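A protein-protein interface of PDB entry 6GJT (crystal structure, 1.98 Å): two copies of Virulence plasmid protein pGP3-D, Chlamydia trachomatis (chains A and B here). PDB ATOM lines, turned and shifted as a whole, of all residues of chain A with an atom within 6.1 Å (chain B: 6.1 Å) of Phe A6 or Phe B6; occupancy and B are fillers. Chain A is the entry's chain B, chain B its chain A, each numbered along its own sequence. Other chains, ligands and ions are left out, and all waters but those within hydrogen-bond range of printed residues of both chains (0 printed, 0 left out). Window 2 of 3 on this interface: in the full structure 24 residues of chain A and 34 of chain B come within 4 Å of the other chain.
Hydrophobic or aromatic side chains of chain A that line the printed part of chain B: Phe A6. Of the 10 printed residues of chain B, 4 touch a printed residue of chain A. Hydrophobic or aromatic side chains of chain B that line the printed part of chain A: Phe B6 and Ala B17. Among the printed residues, 5 pairs touch across the chains.
Of the printed residues of chain B, Phe A6 touches Ser B4, Gly B5 and Phe B6. Of chain A, only Phe A6 (3.9 Å) comes within 4 Å of Phe B6. Printed residues of chain B within 4 Å of Asn A13: Ala B17. Printed residues of chain A within 4 Å of Gly B5: Phe A6. Tyr A7 touches none of the printed residues of chain B.
The backbone carbonyl oxygen of Gly B5 lies within hydrogen-bond range of the backbone NH of Phe B16, 2.9 Å away.
Phe A6 touches Ser B4, but with the chains exchanged Ser A4 does not touch Phe B6 (8.5 Å). Phe A6 touches Gly B5, but with the chains exchanged Gly A5 does not touch Phe B6 (7.4 Å). Phe B6 touches its own counterpart, Phe A6. Positions printed for both chains: 4, 5, 6, 7, 8, 13, 14, 15 and 16. Of the 5 pairs that touch across the chains among the printed residues, 1 has its exchanged pair printed and touching as well.
Among the printed residues, merely in contact across the chains: Phe A6 with Ser B4, Phe A6 with Gly B5, Phe A6 with Phe B6, Asn A13 with Ala B17 and Val A15 with Ala B17.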
ATOM      1  N   SER A   4      32.120   7.642 -26.226  1.00  0.00           N
ATOM      2  CA  SER A   4      30.910   7.862 -25.438  1.00  0.00           C
ATOM      3  C   SER A   4      31.040   9.241 -24.819  1.00  0.00           C
ATOM      4  O   SER A   4      32.128   9.820 -24.790  1.00  0.00           O
ATOM      5  CB  SER A   4      30.706   6.815 -24.348  1.00  0.00           C
ATOM      6  OG  SER A   4      31.750   6.875 -23.389  1.00  0.00           O
ATOM      7  N   GLY A   5      29.919   9.781 -24.383  1.00  0.00           N
ATOM      8  CA  GLY A   5      29.872  11.106 -23.798  1.00  0.00           C
ATOM      9  C   GLY A   5      28.567  11.801 -24.092  1.00  0.00           C
ATOM     10  O   GLY A   5      27.505  11.226 -23.975  1.00  0.00           O
ATOM     11  N   PHE A   6      28.675  13.088 -24.417  1.00  0.00           N
ATOM     12  CA  PHE A   6      27.532  13.968 -24.641  1.00  0.00           C
ATOM     13  C   PHE A   6      27.833  14.821 -25.853  1.00  0.00           C
ATOM     14  O   PHE A   6      28.996  15.030 -26.156  1.00  0.00           O
ATOM     15  CB  PHE A   6      27.283  14.860 -23.463  1.00  0.00           C
ATOM     16  CG  PHE A   6      27.108  14.111 -22.192  1.00  0.00           C
ATOM     17  CD1 PHE A   6      25.840  13.687 -21.801  1.00  0.00           C
ATOM     18  CD2 PHE A   6      28.192  13.806 -21.395  1.00  0.00           C
ATOM     19  CE1 PHE A   6      25.684  12.948 -20.621  1.00  0.00           C
ATOM     20  CE2 PHE A   6      28.038  13.122 -20.210  1.00  0.00           C
ATOM     21  CZ  PHE A   6      26.774  12.677 -19.821  1.00  0.00           C
ATOM     22  N   TYR A   7      26.807  15.157 -26.609  1.00  0.00           N
ATOM     23  CA  TYR A   7      26.980  15.902 -27.854  1.00  0.00           C
ATOM     24  C   TYR A   7      25.710  16.589 -28.264  1.00  0.00           C
ATOM     25  O   TYR A   7      24.628  16.264 -27.770  1.00  0.00           O
ATOM     26  CB  TYR A   7      27.488  15.013 -28.989  1.00  0.00           C
ATOM     27  CG  TYR A   7      26.424  14.334 -29.790  1.00  0.00           C
ATOM     28  CD1 TYR A   7      25.580  13.419 -29.186  1.00  0.00           C
ATOM     29  CD2 TYR A   7      26.275  14.576 -31.141  1.00  0.00           C
ATOM     30  CE1 TYR A   7      24.581  12.787 -29.909  1.00  0.00           C
ATOM     31  CE2 TYR A   7      25.282  13.945 -31.890  1.00  0.00           C
ATOM     32  CZ  TYR A   7      24.446  13.043 -31.256  1.00  0.00           C
ATOM     33  OH  TYR A   7      23.456  12.435 -31.954  1.00  0.00           O
ATOM     34  N   LEU A   8      25.876  17.602 -29.092  1.00  0.00           N
ATOM     35  CA  LEU A   8      24.800  18.432 -29.583  1.00  0.00           C
ATOM     36  C   LEU A   8      24.319  17.882 -30.945  1.00  0.00           C
ATOM     37  O   LEU A   8      25.105  17.587 -31.831  1.00  0.00           O
ATOM     38  CB  LEU A   8      25.338  19.882 -29.571  1.00  0.00           C
ATOM     39  CG  LEU A   8      24.620  21.219 -29.833  1.00  0.00           C
ATOM     40  CD1 LEU A   8      25.187  22.350 -28.960  1.00  0.00           C
ATOM     41  CD2 LEU A   8      24.703  21.625 -31.304  1.00  0.00           C
ATOM     42  N   ASN A  13      20.922  18.443 -26.409  1.00  0.00           N
ATOM     43  CA  ASN A  13      22.121  17.964 -25.706  1.00  0.00           C
ATOM     44  C   ASN A  13      21.946  16.535 -25.294  1.00  0.00           C
ATOM     45  O   ASN A  13      21.259  16.269 -24.302  1.00  0.00           O
ATOM     46  CB  ASN A  13      22.415  18.813 -24.488  1.00  0.00           C
ATOM     47  CG  ASN A  13      23.453  19.796 -24.749  1.00  0.00           C
ATOM     48  OD1 ASN A  13      23.115  20.944 -25.029  1.00  0.00           O
ATOM     49  ND2 ASN A  13      24.704  19.384 -24.711  1.00  0.00           N
ATOM     50  N   CYS A  14      22.620  15.631 -26.003  1.00  0.00           N
ATOM     51  CA  CYS A  14      22.312  14.214 -25.908  1.00  0.00           C
ATOM     52  C   CYS A  14      23.449  13.409 -25.321  1.00  0.00           C
ATOM     53  O   CYS A  14      24.601  13.645 -25.654  1.00  0.00           O
ATOM     54  CB  CYS A  14      22.031  13.650 -27.299  1.00  0.00           C
ATOM     55  SG  CYS A  14      20.749  14.537 -28.223  1.00  0.00           S
ATOM     56  N   VAL A  15      23.124  12.419 -24.521  1.00  0.00           N
ATOM     57  CA  VAL A  15      24.048  11.368 -24.137  1.00  0.00           C
ATOM     58  C   VAL A  15      24.195  10.364 -25.250  1.00  0.00           C
ATOM     59  O   VAL A  15      23.249  10.094 -25.966  1.00  0.00           O
ATOM     60  CB  VAL A  15      23.616  10.646 -22.831  1.00  0.00           C
ATOM     61  CG1 VAL A  15      22.282   9.931 -23.029  1.00  0.00           C
ATOM     62  CG2 VAL A  15      24.680   9.643 -22.349  1.00  0.00           C
ATOM     63  N   PHE A  16      25.412   9.859 -25.451  1.00  0.00           N
ATOM     64  CA  PHE A  16      25.663   8.842 -26.459  1.00  0.00           C
ATOM     65  C   PHE A  16      26.707   7.865 -25.962  1.00  0.00           C
ATOM     66  O   PHE A  16      27.531   8.203 -25.124  1.00  0.00           O
ATOM     67  CB  PHE A  16      26.054   9.457 -27.826  1.00  0.00           C
ATOM     68  CG  PHE A  16      27.498   9.880 -27.938  1.00  0.00           C
ATOM     69  CD1 PHE A  16      27.914  11.120 -27.472  1.00  0.00           C
ATOM     70  CD2 PHE A  16      28.438   9.034 -28.508  1.00  0.00           C
ATOM     71  CE1 PHE A  16      29.245  11.513 -27.579  1.00  0.00           C
ATOM     72  CE2 PHE A  16      29.771   9.398 -28.589  1.00  0.00           C
ATOM     73  CZ  PHE A  16      30.171  10.653 -28.147  1.00  0.00           C
ATOM     74  N   SER B   4      23.272  18.642 -19.782  1.00  0.00           N
ATOM     75  CA  SER B   4      23.411  17.184 -19.667  1.00  0.00           C
ATOM     76  C   SER B   4      24.515  16.831 -18.686  1.00  0.00           C
ATOM     77  O   SER B   4      25.301  17.684 -18.324  1.00  0.00           O
ATOM     78  CB  SER B   4      23.725  16.553 -21.026  1.00  0.00           C
ATOM     79  OG  SER B   4      24.986  16.998 -21.491  1.00  0.00           O
ATOM     80  N   GLY B   5      24.521  15.584 -18.217  1.00  0.00           N
ATOM     81  CA  GLY B   5      25.468  15.127 -17.239  1.00  0.00           C
ATOM     82  C   GLY B   5      24.941  14.054 -16.313  1.00  0.00           C
ATOM     83  O   GLY B   5      24.177  13.188 -16.723  1.00  0.00           O
ATOM     84  N   PHE B   6      25.321  14.159 -15.040  1.00  0.00           N
ATOM     85  CA  PHE B   6      24.829  13.292 -14.000  1.00  0.00           C
ATOM     86  C   PHE B   6      24.375  14.149 -12.823  1.00  0.00           C
ATOM     87  O   PHE B   6      24.838  15.276 -12.655  1.00  0.00           O
ATOM     88  CB  PHE B   6      25.909  12.354 -13.544  1.00  0.00           C
ATOM     89  CG  PHE B   6      26.448  11.500 -14.637  1.00  0.00           C
ATOM     90  CD1 PHE B   6      27.514  11.939 -15.433  1.00  0.00           C
ATOM     91  CD2 PHE B   6      25.877  10.274 -14.903  1.00  0.00           C
ATOM     92  CE1 PHE B   6      27.993  11.150 -16.465  1.00  0.00           C
ATOM     93  CE2 PHE B   6      26.364   9.470 -15.934  1.00  0.00           C
ATOM     94  CZ  PHE B   6      27.419   9.910 -16.718  1.00  0.00           C
ATOM     95  N   TYR B   7      23.418  13.643 -12.046  1.00  0.00           N
ATOM     96  CA  TYR B   7      22.922  14.379 -10.885  1.00  0.00           C
ATOM     97  C   TYR B   7      22.235  13.440  -9.900  1.00  0.00           C
ATOM     98  O   TYR B   7      21.845  12.322 -10.261  1.00  0.00           O
ATOM     99  CB  TYR B   7      21.971  15.515 -11.308  1.00  0.00           C
ATOM    100  CG  TYR B   7      20.530  15.097 -11.460  1.00  0.00           C
ATOM    101  CD1 TYR B   7      20.159  14.121 -12.389  1.00  0.00           C
ATOM    102  CD2 TYR B   7      19.532  15.672 -10.664  1.00  0.00           C
ATOM    103  CE1 TYR B   7      18.846  13.744 -12.536  1.00  0.00           C
ATOM    104  CE2 TYR B   7      18.208  15.292 -10.794  1.00  0.00           C
ATOM    105  CZ  TYR B   7      17.877  14.332 -11.735  1.00  0.00           C
ATOM    106  OH  TYR B   7      16.574  13.950 -11.854  1.00  0.00           O
ATOM    107  N   LEU B   8      22.090  13.923  -8.664  1.00  0.00           N
ATOM    108  CA  LEU B   8      21.413  13.178  -7.607  1.00  0.00           C
ATOM    109  C   LEU B   8      19.948  13.575  -7.532  1.00  0.00           C
ATOM    110  O   LEU B   8      19.623  14.760  -7.482  1.00  0.00           O
ATOM    111  CB  LEU B   8      22.059  13.392  -6.227  1.00  0.00           C
ATOM    112  CG  LEU B   8      23.368  12.727  -5.838  1.00  0.00           C
ATOM    113  CD1 LEU B   8      24.402  13.177  -6.843  1.00  0.00           C
ATOM    114  CD2 LEU B   8      23.773  13.055  -4.401  1.00  0.00           C
ATOM    115  N   ASN B  13      21.813   8.291  -8.210  1.00  0.00           N
ATOM    116  CA  ASN B  13      22.743   8.976  -9.121  1.00  0.00           C
ATOM    117  C   ASN B  13      22.333   8.710 -10.576  1.00  0.00           C
ATOM    118  O   ASN B  13      22.482   7.583 -11.080  1.00  0.00           O
ATOM    119  CB  ASN B  13      24.171   8.485  -8.871  1.00  0.00           C
ATOM    120  CG  ASN B  13      25.233   9.473  -9.362  1.00  0.00           C
ATOM    121  OD1 ASN B  13      24.940  10.463 -10.060  1.00  0.00           O
ATOM    122  ND2 ASN B  13      26.485   9.190  -9.024  1.00  0.00           N
ATOM    123  N   CYS B  14      21.805   9.742 -11.234  1.00  0.00           N
ATOM    124  CA  CYS B  14      21.146   9.584 -12.517  1.00  0.00           C
ATOM    125  C   CYS B  14      21.859  10.295 -13.649  1.00  0.00           C
ATOM    126  O   CYS B  14      22.332  11.413 -13.468  1.00  0.00           O
ATOM    127  CB  CYS B  14      19.748  10.173 -12.452  1.00  0.00           C
ATOM    128  SG  CYS B  14      18.748   9.551 -11.109  1.00  0.00           S
ATOM    129  N   VAL B  15      21.891   9.657 -14.816  1.00  0.00           N
ATOM    130  CA  VAL B  15      22.270  10.349 -16.059  1.00  0.00           C
ATOM    131  C   VAL B  15      21.103  11.196 -16.532  1.00  0.00           C
ATOM    132  O   VAL B  15      19.956  10.801 -16.374  1.00  0.00           O
ATOM    133  CB  VAL B  15      22.720   9.369 -17.157  1.00  0.00           C
ATOM    134  CG1 VAL B  15      21.587   8.441 -17.550  1.00  0.00           C
ATOM    135  CG2 VAL B  15      23.256  10.100 -18.381  1.00  0.00           C
ATOM    136  N   PHE B  16      21.384  12.365 -17.084  1.00  0.00           N
ATOM    137  CA  PHE B  16      20.340  13.193 -17.672  1.00  0.00           C
ATOM    138  C   PHE B  16      20.856  13.909 -18.920  1.00  0.00           C
ATOM    139  O   PHE B  16      22.059  14.104 -19.058  1.00  0.00           O
ATOM    140  CB  PHE B  16      19.771  14.185 -16.651  1.00  0.00           C
ATOM    141  CG  PHE B  16      20.609  15.428 -16.444  1.00  0.00           C
ATOM    142  CD1 PHE B  16      21.671  15.429 -15.539  1.00  0.00           C
ATOM    143  CD2 PHE B  16      20.311  16.592 -17.111  1.00  0.00           C
ATOM    144  CE1 PHE B  16      22.432  16.572 -15.322  1.00  0.00           C
ATOM    145  CE2 PHE B  16      21.067  17.739 -16.910  1.00  0.00           C
ATOM    146  CZ  PHE B  16      22.121  17.731 -15.993  1.00  0.00           C
ATOM    147  N   ALA B  17      19.929  14.242 -19.818  1.00  0.00           N
ATOM    148  CA  ALA B  17      20.184  14.868 -21.106  1.00  0.00           C
ATOM    149  C   ALA B  17      18.862  15.215 -21.804  1.00  0.00           C
ATOM    150  O   ALA B  17      17.809  14.820 -21.363  1.00  0.00           O
ATOM    151  CB  ALA B  17      21.010  13.939 -21.995  1.00  0.00           C
